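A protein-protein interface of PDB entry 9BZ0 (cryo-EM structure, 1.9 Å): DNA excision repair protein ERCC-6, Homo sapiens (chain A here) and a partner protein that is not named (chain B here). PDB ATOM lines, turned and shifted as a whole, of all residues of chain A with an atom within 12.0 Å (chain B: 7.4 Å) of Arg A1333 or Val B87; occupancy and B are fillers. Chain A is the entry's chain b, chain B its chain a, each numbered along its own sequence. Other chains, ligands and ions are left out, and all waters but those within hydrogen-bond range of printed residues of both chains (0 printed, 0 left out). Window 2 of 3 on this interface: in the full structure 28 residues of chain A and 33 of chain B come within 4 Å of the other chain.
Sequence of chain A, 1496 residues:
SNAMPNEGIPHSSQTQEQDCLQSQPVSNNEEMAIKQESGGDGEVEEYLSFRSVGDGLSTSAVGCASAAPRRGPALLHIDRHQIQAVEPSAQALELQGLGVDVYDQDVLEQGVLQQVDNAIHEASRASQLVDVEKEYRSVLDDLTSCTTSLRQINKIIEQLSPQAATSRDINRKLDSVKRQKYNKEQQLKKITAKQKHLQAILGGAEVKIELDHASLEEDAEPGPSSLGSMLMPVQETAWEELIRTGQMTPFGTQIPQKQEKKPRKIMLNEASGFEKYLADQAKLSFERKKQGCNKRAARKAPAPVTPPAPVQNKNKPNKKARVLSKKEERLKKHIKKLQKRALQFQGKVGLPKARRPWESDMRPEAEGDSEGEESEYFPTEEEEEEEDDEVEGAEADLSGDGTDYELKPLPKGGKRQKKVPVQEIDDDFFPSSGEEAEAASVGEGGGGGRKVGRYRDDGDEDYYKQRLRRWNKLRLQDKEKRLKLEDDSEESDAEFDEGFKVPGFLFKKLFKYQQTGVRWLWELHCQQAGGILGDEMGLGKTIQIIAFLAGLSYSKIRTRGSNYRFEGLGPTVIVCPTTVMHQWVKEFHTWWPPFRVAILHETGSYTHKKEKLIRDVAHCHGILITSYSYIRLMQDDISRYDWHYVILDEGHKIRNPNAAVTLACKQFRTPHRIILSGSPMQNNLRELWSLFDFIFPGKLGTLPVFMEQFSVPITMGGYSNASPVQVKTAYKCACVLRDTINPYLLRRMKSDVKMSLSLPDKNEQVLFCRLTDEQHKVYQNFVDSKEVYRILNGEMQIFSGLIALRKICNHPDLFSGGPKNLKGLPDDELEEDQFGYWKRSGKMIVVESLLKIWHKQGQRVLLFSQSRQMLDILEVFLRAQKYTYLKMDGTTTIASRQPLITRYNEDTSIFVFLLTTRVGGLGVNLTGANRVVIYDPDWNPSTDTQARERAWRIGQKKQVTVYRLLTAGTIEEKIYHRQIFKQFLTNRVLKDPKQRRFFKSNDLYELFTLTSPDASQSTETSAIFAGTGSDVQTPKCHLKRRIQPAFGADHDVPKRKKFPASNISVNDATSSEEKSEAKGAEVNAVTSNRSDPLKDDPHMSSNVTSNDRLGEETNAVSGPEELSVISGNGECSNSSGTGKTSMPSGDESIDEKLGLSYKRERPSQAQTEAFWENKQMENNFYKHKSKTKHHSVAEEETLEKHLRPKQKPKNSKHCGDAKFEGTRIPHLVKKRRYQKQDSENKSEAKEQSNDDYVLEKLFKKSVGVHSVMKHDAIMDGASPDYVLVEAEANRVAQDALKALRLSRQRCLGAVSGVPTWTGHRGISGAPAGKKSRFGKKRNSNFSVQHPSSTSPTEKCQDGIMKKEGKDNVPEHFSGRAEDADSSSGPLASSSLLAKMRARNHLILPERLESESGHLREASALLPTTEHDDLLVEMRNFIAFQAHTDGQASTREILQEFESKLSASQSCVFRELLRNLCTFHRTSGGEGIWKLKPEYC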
ATOM      1  N   SER A1332     -28.340 -20.174  23.960  1.00  0.00           N
ATOM      2  CA  SER A1332     -27.180 -21.032  24.163  1.00  0.00           C
ATOM      3  C   SER A1332     -27.436 -22.434  23.641  1.00  0.00           C
ATOM      4  O   SER A1332     -28.476 -23.027  23.910  1.00  0.00           O
ATOM      5  CB  SER A1332     -26.809 -21.088  25.646  1.00  0.00           C
ATOM      6  OG  SER A1332     -26.565 -19.792  26.161  1.00  0.00           O
ATOM      7  N   ARG A1333     -26.476 -22.958  22.887  1.00  0.00           N
ATOM      8  CA  ARG A1333     -26.589 -24.316  22.371  1.00  0.00           C
ATOM      9  C   ARG A1333     -26.394 -25.358  23.463  1.00  0.00           C
ATOM     10  O   ARG A1333     -26.946 -26.456  23.373  1.00  0.00           O
ATOM     11  CB  ARG A1333     -25.582 -24.526  21.249  1.00  0.00           C
ATOM     12  CG  ARG A1333     -25.677 -25.862  20.566  1.00  0.00           C
ATOM     13  CD  ARG A1333     -24.810 -25.875  19.332  1.00  0.00           C
ATOM     14  NE  ARG A1333     -24.993 -27.089  18.553  1.00  0.00           N
ATOM     15  CZ  ARG A1333     -24.955 -27.138  17.231  1.00  0.00           C
ATOM     16  NH1 ARG A1333     -25.232 -28.283  16.616  1.00  0.00           N
ATOM     17  NH2 ARG A1333     -24.626 -26.079  16.510  1.00  0.00           N
ATOM     18  N   PHE A1334     -25.619 -25.037  24.493  1.00  0.00           N
ATOM     19  CA  PHE A1334     -25.238 -25.988  25.524  1.00  0.00           C
ATOM     20  C   PHE A1334     -25.608 -25.446  26.894  1.00  0.00           C
ATOM     21  O   PHE A1334     -25.695 -24.237  27.101  1.00  0.00           O
ATOM     22  CB  PHE A1334     -23.745 -26.293  25.502  1.00  0.00           C
ATOM     23  CG  PHE A1334     -23.228 -26.723  24.173  1.00  0.00           C
ATOM     24  CD1 PHE A1334     -23.377 -28.020  23.751  1.00  0.00           C
ATOM     25  CD2 PHE A1334     -22.566 -25.841  23.357  1.00  0.00           C
ATOM     26  CE1 PHE A1334     -22.893 -28.421  22.537  1.00  0.00           C
ATOM     27  CE2 PHE A1334     -22.079 -26.241  22.141  1.00  0.00           C
ATOM     28  CZ  PHE A1334     -22.246 -27.532  21.732  1.00  0.00           C
ATOM     29  N   GLY A1335     -25.824 -26.358  27.826  1.00  0.00           N
ATOM     30  CA  GLY A1335     -26.195 -26.014  29.172  1.00  0.00           C
ATOM     31  C   GLY A1335     -27.661 -25.719  29.362  1.00  0.00           C
ATOM     32  O   GLY A1335     -28.065 -25.363  30.475  1.00  0.00           O
ATOM     33  N   LYS A1336     -28.472 -25.860  28.312  1.00  0.00           N
ATOM     34  CA  LYS A1336     -29.884 -25.509  28.381  1.00  0.00           C
ATOM     35  C   LYS A1336     -30.685 -26.485  29.233  1.00  0.00           C
ATOM     36  O   LYS A1336     -31.759 -26.123  29.723  1.00  0.00           O
ATOM     37  CB  LYS A1336     -30.473 -25.442  26.971  1.00  0.00           C
ATOM     38  CG  LYS A1336     -31.787 -24.686  26.880  1.00  0.00           C
ATOM     39  CD  LYS A1336     -32.234 -24.523  25.437  1.00  0.00           C
ATOM     40  CE  LYS A1336     -33.461 -23.632  25.343  1.00  0.00           C
ATOM     41  NZ  LYS A1336     -34.665 -24.298  25.912  1.00  0.00           N
ATOM     42  N   LYS A1337     -30.189 -27.706  29.425  1.00  0.00           N
ATOM     43  CA  LYS A1337     -30.897 -28.725  30.184  1.00  0.00           C
ATOM     44  C   LYS A1337     -29.965 -29.355  31.207  1.00  0.00           C
ATOM     45  O   LYS A1337     -28.786 -29.592  30.930  1.00  0.00           O
ATOM     46  CB  LYS A1337     -31.467 -29.812  29.264  1.00  0.00           C
ATOM     47  CG  LYS A1337     -32.470 -29.304  28.241  1.00  0.00           C
ATOM     48  CD  LYS A1337     -33.065 -30.450  27.439  1.00  0.00           C
ATOM     49  CE  LYS A1337     -33.986 -29.938  26.343  1.00  0.00           C
ATOM     50  NZ  LYS A1337     -34.569 -31.053  25.547  1.00  0.00           N
ATOM     51  N   ARG A1338     -30.510 -29.626  32.387  1.00  0.00           N
ATOM     52  CA  ARG A1338     -29.825 -30.416  33.394  1.00  0.00           C
ATOM     53  C   ARG A1338     -29.911 -31.900  33.063  1.00  0.00           C
ATOM     54  O   ARG A1338     -30.862 -32.365  32.429  1.00  0.00           O
ATOM     55  CB  ARG A1338     -30.431 -30.162  34.775  1.00  0.00           C
ATOM     56  CG  ARG A1338     -30.144 -28.786  35.349  1.00  0.00           C
ATOM     57  CD  ARG A1338     -30.853 -28.600  36.681  1.00  0.00           C
ATOM     58  NE  ARG A1338     -30.488 -27.348  37.333  1.00  0.00           N
ATOM     59  CZ  ARG A1338     -29.521 -27.226  38.232  1.00  0.00           C
ATOM     60  NH1 ARG A1338     -29.315 -26.044  38.807  1.00  0.00           N
ATOM     61  NH2 ARG A1338     -28.741 -28.246  38.552  1.00  0.00           N
ATOM     62  N   SER A1389     -23.620 -25.353  35.693  1.00  0.00           N
ATOM     63  CA  SER A1389     -22.374 -24.913  35.090  1.00  0.00           C
ATOM     64  C   SER A1389     -22.239 -23.402  35.117  1.00  0.00           C
ATOM     65  O   SER A1389     -21.148 -22.884  35.348  1.00  0.00           O
ATOM     66  CB  SER A1389     -22.276 -25.424  33.658  1.00  0.00           C
ATOM     67  OG  SER A1389     -21.136 -24.901  33.009  1.00  0.00           O
ATOM     68  N   SER A1390     -23.312 -22.679  34.820  1.00  0.00           N
ATOM     69  CA  SER A1390     -23.216 -21.226  34.742  1.00  0.00           C
ATOM     70  C   SER A1390     -22.754 -20.576  36.042  1.00  0.00           C
ATOM     71  O   SER A1390     -21.937 -19.651  36.006  1.00  0.00           O
ATOM     72  CB  SER A1390     -24.563 -20.648  34.321  1.00  0.00           C
ATOM     73  OG  SER A1390     -25.008 -21.235  33.113  1.00  0.00           O
ATOM     74  N   LEU A1393     -18.927 -21.673  36.576  1.00  0.00           N
ATOM     75  CA  LEU A1393     -18.174 -20.831  35.664  1.00  0.00           C
ATOM     76  C   LEU A1393     -18.075 -19.399  36.156  1.00  0.00           C
ATOM     77  O   LEU A1393     -17.020 -18.772  36.030  1.00  0.00           O
ATOM     78  CB  LEU A1393     -18.817 -20.866  34.284  1.00  0.00           C
ATOM     79  CG  LEU A1393     -18.640 -22.154  33.484  1.00  0.00           C
ATOM     80  CD1 LEU A1393     -19.548 -22.140  32.273  1.00  0.00           C
ATOM     81  CD2 LEU A1393     -17.210 -22.350  33.068  1.00  0.00           C
ATOM     82  N   GLU B  39     -16.609 -37.511  10.754  1.00  0.00           N
ATOM     83  CA  GLU B  39     -15.750 -36.605  10.001  1.00  0.00           C
ATOM     84  C   GLU B  39     -14.315 -36.639  10.513  1.00  0.00           C
ATOM     85  O   GLU B  39     -14.072 -36.489  11.712  1.00  0.00           O
ATOM     86  CB  GLU B  39     -16.311 -35.191  10.097  1.00  0.00           C
ATOM     87  CG  GLU B  39     -15.527 -34.147   9.352  1.00  0.00           C
ATOM     88  CD  GLU B  39     -16.271 -32.839   9.245  1.00  0.00           C
ATOM     89  OE1 GLU B  39     -16.958 -32.463  10.212  1.00  0.00           O
ATOM     90  OE2 GLU B  39     -16.170 -32.181   8.190  1.00  0.00           O
ATOM     91  N   ILE B  41     -11.395 -34.955  11.401  1.00  0.00           N
ATOM     92  CA  ILE B  41     -10.769 -33.683  11.726  1.00  0.00           C
ATOM     93  C   ILE B  41      -9.354 -33.861  12.261  1.00  0.00           C
ATOM     94  O   ILE B  41      -8.459 -33.090  11.920  1.00  0.00           O
ATOM     95  CB  ILE B  41     -11.645 -32.890  12.714  1.00  0.00           C
ATOM     96  CG1 ILE B  41     -12.998 -32.596  12.081  1.00  0.00           C
ATOM     97  CG2 ILE B  41     -10.976 -31.608  13.106  1.00  0.00           C
ATOM     98  CD1 ILE B  41     -12.898 -31.836  10.798  1.00  0.00           C
ATOM     99  N   GLU B  55     -28.113 -35.858  26.821  1.00  0.00           N
ATOM    100  CA  GLU B  55     -28.864 -36.281  25.654  1.00  0.00           C
ATOM    101  C   GLU B  55     -28.144 -37.316  24.810  1.00  0.00           C
ATOM    102  O   GLU B  55     -28.793 -37.984  24.004  1.00  0.00           O
ATOM    103  CB  GLU B  55     -29.206 -35.081  24.764  1.00  0.00           C
ATOM    104  CG  GLU B  55     -30.014 -34.011  25.458  1.00  0.00           C
ATOM    105  CD  GLU B  55     -30.627 -33.023  24.486  1.00  0.00           C
ATOM    106  OE1 GLU B  55     -29.895 -32.511  23.614  1.00  0.00           O
ATOM    107  OE2 GLU B  55     -31.844 -32.759  24.593  1.00  0.00           O
ATOM    108  N   ARG B  57     -26.176 -36.595  22.468  1.00  0.00           N
ATOM    109  CA  ARG B  57     -26.049 -36.056  21.128  1.00  0.00           C
ATOM    110  C   ARG B  57     -24.606 -35.741  20.774  1.00  0.00           C
ATOM    111  O   ARG B  57     -24.198 -35.914  19.625  1.00  0.00           O
ATOM    112  CB  ARG B  57     -26.921 -34.819  20.992  1.00  0.00           C
ATOM    113  CG  ARG B  57     -26.873 -34.222  19.638  1.00  0.00           C
ATOM    114  CD  ARG B  57     -27.890 -33.147  19.452  1.00  0.00           C
ATOM    115  NE  ARG B  57     -27.763 -32.591  18.114  1.00  0.00           N
ATOM    116  CZ  ARG B  57     -28.454 -31.561  17.659  1.00  0.00           C
ATOM    117  NH1 ARG B  57     -28.198 -31.099  16.441  1.00  0.00           N
ATOM    118  NH2 ARG B  57     -29.409 -31.001  18.377  1.00  0.00           N
ATOM    119  N   TYR B  58     -23.824 -35.250  21.731  1.00  0.00           N
ATOM    120  CA  TYR B  58     -22.507 -34.701  21.453  1.00  0.00           C
ATOM    121  C   TYR B  58     -21.403 -35.600  21.973  1.00  0.00           C
ATOM    122  O   TYR B  58     -21.532 -36.215  23.031  1.00  0.00           O
ATOM    123  CB  TYR B  58     -22.364 -33.309  22.038  1.00  0.00           C
ATOM    124  CG  TYR B  58     -23.287 -32.376  21.356  1.00  0.00           C
ATOM    125  CD1 TYR B  58     -23.051 -31.979  20.063  1.00  0.00           C
ATOM    126  CD2 TYR B  58     -24.417 -31.922  21.981  1.00  0.00           C
ATOM    127  CE1 TYR B  58     -23.901 -31.157  19.422  1.00  0.00           C
ATOM    128  CE2 TYR B  58     -25.273 -31.089  21.348  1.00  0.00           C
ATOM    129  CZ  TYR B  58     -25.013 -30.710  20.070  1.00  0.00           C
ATOM    130  OH  TYR B  58     -25.873 -29.860  19.436  1.00  0.00           O
ATOM    131  N   MET B  59     -20.311 -35.655  21.223  1.00  0.00           N
ATOM    132  CA  MET B  59     -19.133 -36.419  21.588  1.00  0.00           C
ATOM    133  C   MET B  59     -17.923 -35.511  21.503  1.00  0.00           C
ATOM    134  O   MET B  59     -17.659 -34.923  20.452  1.00  0.00           O
ATOM    135  CB  MET B  59     -18.975 -37.631  20.680  1.00  0.00           C
ATOM    136  CG  MET B  59     -17.817 -38.508  21.012  1.00  0.00           C
ATOM    137  SD  MET B  59     -17.898 -40.004  20.044  1.00  0.00           S
ATOM    138  CE  MET B  59     -17.480 -39.383  18.434  1.00  0.00           C
ATOM    139  N   VAL B  69     -11.963 -31.926  19.545  1.00  0.00           N
ATOM    140  CA  VAL B  69     -13.026 -31.785  18.559  1.00  0.00           C
ATOM    141  C   VAL B  69     -14.353 -32.128  19.214  1.00  0.00           C
ATOM    142  O   VAL B  69     -14.442 -33.079  19.994  1.00  0.00           O
ATOM    143  CB  VAL B  69     -12.781 -32.663  17.320  1.00  0.00           C
ATOM    144  CG1 VAL B  69     -13.808 -32.362  16.262  1.00  0.00           C
ATOM    145  CG2 VAL B  69     -11.397 -32.436  16.786  1.00  0.00           C
ATOM    146  N   LEU B  70     -15.378 -31.338  18.917  1.00  0.00           N
ATOM    147  CA  LEU B  70     -16.742 -31.578  19.369  1.00  0.00           C
ATOM    148  C   LEU B  70     -17.618 -31.975  18.185  1.00  0.00           C
ATOM    149  O   LEU B  70     -17.717 -31.231  17.208  1.00  0.00           O
ATOM    150  CB  LEU B  70     -17.285 -30.340  20.073  1.00  0.00           C
ATOM    151  CG  LEU B  70     -18.719 -30.361  20.567  1.00  0.00           C
ATOM    152  CD1 LEU B  70     -18.948 -31.543  21.475  1.00  0.00           C
ATOM    153  CD2 LEU B  70     -18.989 -29.085  21.300  1.00  0.00           C
ATOM    154  N   TYR B  71     -18.247 -33.141  18.277  1.00  0.00           N
ATOM    155  CA  TYR B  71     -19.040 -33.727  17.208  1.00  0.00           C
ATOM    156  C   TYR B  71     -20.517 -33.767  17.572  1.00  0.00           C
ATOM    157  O   TYR B  71     -20.877 -33.945  18.734  1.00  0.00           O
ATOM    158  CB  TYR B  71     -18.616 -35.158  16.920  1.00  0.00           C
ATOM    159  CG  TYR B  71     -17.282 -35.343  16.280  1.00  0.00           C
ATOM    160  CD1 TYR B  71     -17.124 -35.238  14.923  1.00  0.00           C
ATOM    161  CD2 TYR B  71     -16.193 -35.705  17.037  1.00  0.00           C
ATOM    162  CE1 TYR B  71     -15.912 -35.415  14.350  1.00  0.00           C
ATOM    163  CE2 TYR B  71     -14.985 -35.903  16.466  1.00  0.00           C
ATOM    164  CZ  TYR B  71     -14.848 -35.756  15.124  1.00  0.00           C
ATOM    165  OH  TYR B  71     -13.630 -35.972  14.540  1.00  0.00           O
ATOM    166  N   ASP B  72     -21.369 -33.606  16.566  1.00  0.00           N
ATOM    167  CA  ASP B  72     -22.801 -33.849  16.689  1.00  0.00           C
ATOM    168  C   ASP B  72     -23.125 -35.200  16.071  1.00  0.00           C
ATOM    169  O   ASP B  72     -22.823 -35.439  14.902  1.00  0.00           O
ATOM    170  CB  ASP B  72     -23.592 -32.742  16.001  1.00  0.00           C
ATOM    171  CG  ASP B  72     -25.084 -32.948  16.080  1.00  0.00           C
ATOM    172  OD1 ASP B  72     -25.539 -33.843  16.817  1.00  0.00           O
ATOM    173  OD2 ASP B  72     -25.814 -32.205  15.397  1.00  0.00           O
ATOM    174  N   LEU B  73     -23.732 -36.081  16.854  1.00  0.00           N
ATOM    175  CA  LEU B  73     -24.017 -37.437  16.416  1.00  0.00           C
ATOM    176  C   LEU B  73     -25.370 -37.608  15.739  1.00  0.00           C
ATOM    177  O   LEU B  73     -25.588 -38.637  15.100  1.00  0.00           O
ATOM    178  CB  LEU B  73     -23.914 -38.396  17.595  1.00  0.00           C
ATOM    179  CG  LEU B  73     -22.565 -38.433  18.296  1.00  0.00           C
ATOM    180  CD1 LEU B  73     -22.615 -39.413  19.422  1.00  0.00           C
ATOM    181  CD2 LEU B  73     -21.520 -38.845  17.330  1.00  0.00           C
ATOM    182  N   CYS B  84     -21.369 -37.779  10.863  1.00  0.00           N
ATOM    183  CA  CYS B  84     -21.271 -37.068  12.135  1.00  0.00           C
ATOM    184  C   CYS B  84     -20.284 -35.920  12.003  1.00  0.00           C
ATOM    185  O   CYS B  84     -19.070 -36.118  12.013  1.00  0.00           O
ATOM    186  CB  CYS B  84     -20.871 -38.022  13.251  1.00  0.00           C
ATOM    187  SG  CYS B  84     -21.908 -39.476  13.400  1.00  0.00           S
ATOM    188  N   LYS B  85     -20.813 -34.712  11.884  1.00  0.00           N
ATOM    189  CA  LYS B  85     -20.019 -33.531  11.598  1.00  0.00           C
ATOM    190  C   LYS B  85     -19.425 -32.930  12.858  1.00  0.00           C
ATOM    191  O   LYS B  85     -19.975 -33.056  13.953  1.00  0.00           O
ATOM    192  CB  LYS B  85     -20.862 -32.498  10.865  1.00  0.00           C
ATOM    193  CG  LYS B  85     -21.113 -32.857   9.419  1.00  0.00           C
ATOM    194  CD  LYS B  85     -21.906 -31.781   8.711  1.00  0.00           C
ATOM    195  CE  LYS B  85     -22.107 -32.125   7.247  1.00  0.00           C
ATOM    196  NZ  LYS B  85     -22.902 -31.085   6.538  1.00  0.00           N
ATOM    197  N   ALA B  86     -18.281 -32.275  12.696  1.00  0.00           N
ATOM    198  CA  ALA B  86     -17.670 -31.513  13.775  1.00  0.00           C
ATOM    199  C   ALA B  86     -18.342 -30.162  13.945  1.00  0.00           C
ATOM    200  O   ALA B  86     -18.339 -29.336  13.031  1.00  0.00           O
ATOM    201  CB  ALA B  86     -16.184 -31.331  13.505  1.00  0.00           C
ATOM    202  N   VAL B  87     -18.922 -29.947  15.121  1.00  0.00           N
ATOM    203  CA  VAL B  87     -19.548 -28.672  15.438  1.00  0.00           C
ATOM    204  C   VAL B  87     -18.500 -27.583  15.594  1.00  0.00           C
ATOM    205  O   VAL B  87     -18.612 -26.504  15.008  1.00  0.00           O
ATOM    206  CB  VAL B  87     -20.407 -28.803  16.704  1.00  0.00           C
ATOM    207  CG1 VAL B  87     -21.103 -27.501  17.002  1.00  0.00           C
ATOM    208  CG2 VAL B  87     -21.408 -29.910  16.544  1.00  0.00           C
ATOM    209  N   CYS B  88     -17.467 -27.849  16.384  1.00  0.00           N
ATOM    210  CA  CYS B  88     -16.417 -26.875  16.634  1.00  0.00           C
ATOM    211  C   CYS B  88     -15.198 -27.597  17.180  1.00  0.00           C
ATOM    212  O   CYS B  88     -15.266 -28.758  17.580  1.00  0.00           O
ATOM    213  CB  CYS B  88     -16.884 -25.797  17.609  1.00  0.00           C
ATOM    214  SG  CYS B  88     -17.501 -26.427  19.168  1.00  0.00           S
ATOM    215  N   SER B  89     -14.076 -26.889  17.192  1.00  0.00           N
ATOM    216  CA  SER B  89     -12.792 -27.477  17.519  1.00  0.00           C
ATOM    217  C   SER B  89     -11.948 -26.481  18.290  1.00  0.00           C
ATOM    218  O   SER B  89     -12.003 -25.278  18.028  1.00  0.00           O
ATOM    219  CB  SER B  89     -12.051 -27.905  16.256  1.00  0.00           C
ATOM    220  OG  SER B  89     -10.778 -28.436  16.569  1.00  0.00           O
ATOM    221  N   THR B 112     -24.210 -29.671  29.972  1.00  0.00           N
ATOM    222  CA  THR B 112     -23.259 -29.623  28.878  1.00  0.00           C
ATOM    223  C   THR B 112     -22.487 -28.321  28.790  1.00  0.00           C
ATOM    224  O   THR B 112     -21.655 -28.181  27.894  1.00  0.00           O
ATOM    225  CB  THR B 112     -23.978 -29.856  27.565  1.00  0.00           C
ATOM    226  OG1 THR B 112     -24.953 -28.830  27.376  1.00  0.00           O
ATOM    227  CG2 THR B 112     -24.685 -31.137  27.621  1.00  0.00           C
ATOM    228  N   THR B 129     -18.319 -24.296  27.362  1.00  0.00           N
ATOM    229  CA  THR B 129     -18.630 -24.930  26.085  1.00  0.00           C
ATOM    230  C   THR B 129     -19.231 -23.951  25.089  1.00  0.00           C
ATOM    231  O   THR B 129     -18.986 -24.071  23.888  1.00  0.00           O
ATOM    232  CB  THR B 129     -19.586 -26.096  26.298  1.00  0.00           C
ATOM    233  OG1 THR B 129     -19.136 -26.879  27.405  1.00  0.00           O
ATOM    234  CG2 THR B 129     -19.612 -26.971  25.088  1.00  0.00           C
ATOM    235  N   ASN B 130     -20.016 -22.986  25.556  1.00  0.00           N
ATOM    236  CA  ASN B 130     -20.634 -22.037  24.640  1.00  0.00           C
ATOM    237  C   ASN B 130     -19.609 -21.132  23.977  1.00  0.00           C
ATOM    238  O   ASN B 130     -19.826 -20.677  22.853  1.00  0.00           O
ATOM    239  CB  ASN B 130     -21.666 -21.201  25.380  1.00  0.00           C
ATOM    240  CG  ASN B 130     -22.887 -21.986  25.742  1.00  0.00           C
ATOM    241  OD1 ASN B 130     -23.576 -22.512  24.877  1.00  0.00           O
ATOM    242  ND2 ASN B 130     -23.177 -22.063  27.028  1.00  0.00           N
ATOM    243  N   LEU B 132     -15.915 -21.790  24.250  1.00  0.00           N
ATOM    244  CA  LEU B 132     -14.622 -22.455  24.126  1.00  0.00           C
ATOM    245  C   LEU B 132     -13.473 -21.639  24.703  1.00  0.00           C
ATOM    246  O   LEU B 132     -12.356 -21.669  24.188  1.00  0.00           O
ATOM    247  CB  LEU B 132     -14.339 -22.840  22.677  1.00  0.00           C
ATOM    248  CG  LEU B 132     -15.375 -23.730  21.996  1.00  0.00           C
ATOM    249  CD1 LEU B 132     -14.945 -24.044  20.586  1.00  0.00           C
ATOM    250  CD2 LEU B 132     -15.555 -25.010  22.769  1.00  0.00           C
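The backbone carbonyl oxygen (O) of Thr B112 sits at hydrogen-bond distance from the side-chain hydroxyl (OG1) of Thr B129.
O of Leu B70 sits at hydrogen-bond distance from N of Val B87.
The backbone NH (N) of Leu B70 lies within hydrogen-bond range of the backbone carbonyl oxygen (O) of Cys B88, at 2.9 Å.
No residue of chain A comes within 4 Å of Asp B72.
No residue of chain A comes within 4 Å of Cys B88.
Thr B112 touches just these residues of chain A: Phe A1334 (3.4 Å) and Gly A1335 (2.7 Å).
Asn B130 touches three residues of chain A.
Of the printed residues of chain A, Glu B55 touches Lys A1337.
Printed residues of chain A within 4 Å of Thr B129: Phe A1334 (3.6 Å).
The nearest residue of chain B that does not touch Arg A1333 is Arg B57 (4.1 Å).
The nearest residue of chain A that does not touch Val B87 is Phe A1334 (4.9 Å).
The nearest printed residue of chain A that does not touch Glu B55 is Arg A1333 (6.7 Å).
Printed residues of chain B that touch a printed residue of chain A: Glu B55, Tyr B58, Leu B70, Val B87, Thr B112, Thr B129 and Asn B130.
Hydrophobic or aromatic side chains of chain B within 4 Å of the printed part of chain A: Tyr B58, Leu B70 and Val B87.
Of the 10 printed residues of chain A, 5 touch a printed residue of chain B.
Among the printed residues, 11 pairs touch across the chains.
Among the printed residues, Asp or Glu carboxylates within 4 Å of a Lys or Arg side-chain nitrogen of the other chain: Lys A1337 with Glu B55 (3.4 Å).
OE2 of Glu B55 is in salt-bridge range of NZ of Lys A1337, at 3.4 Å.
N of Phe A1334 lies within hydrogen-bond range of OD1 of Asn B130, 3.3 Å away.
The backbone NH of Gly A1335 is in hydrogen-bond range of the side-chain hydroxyl of Thr B112, at 2.7 Å.
The guanidinium group (NE) of Arg A1333 lies within hydrogen-bond range of the side-chain hydroxyl (OH) of Tyr B58 (3.0 Å).
Among the printed residues, merely in contact across the chains: Phe A1334 with Thr B112, Arg A1333 with Asn B130, Phe A1334 with Thr B129, Ser A1332 with Asn B130, Phe A1334 with Leu B70, Phe A1334 with Tyr B58 and Arg A1333 with Val B87.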
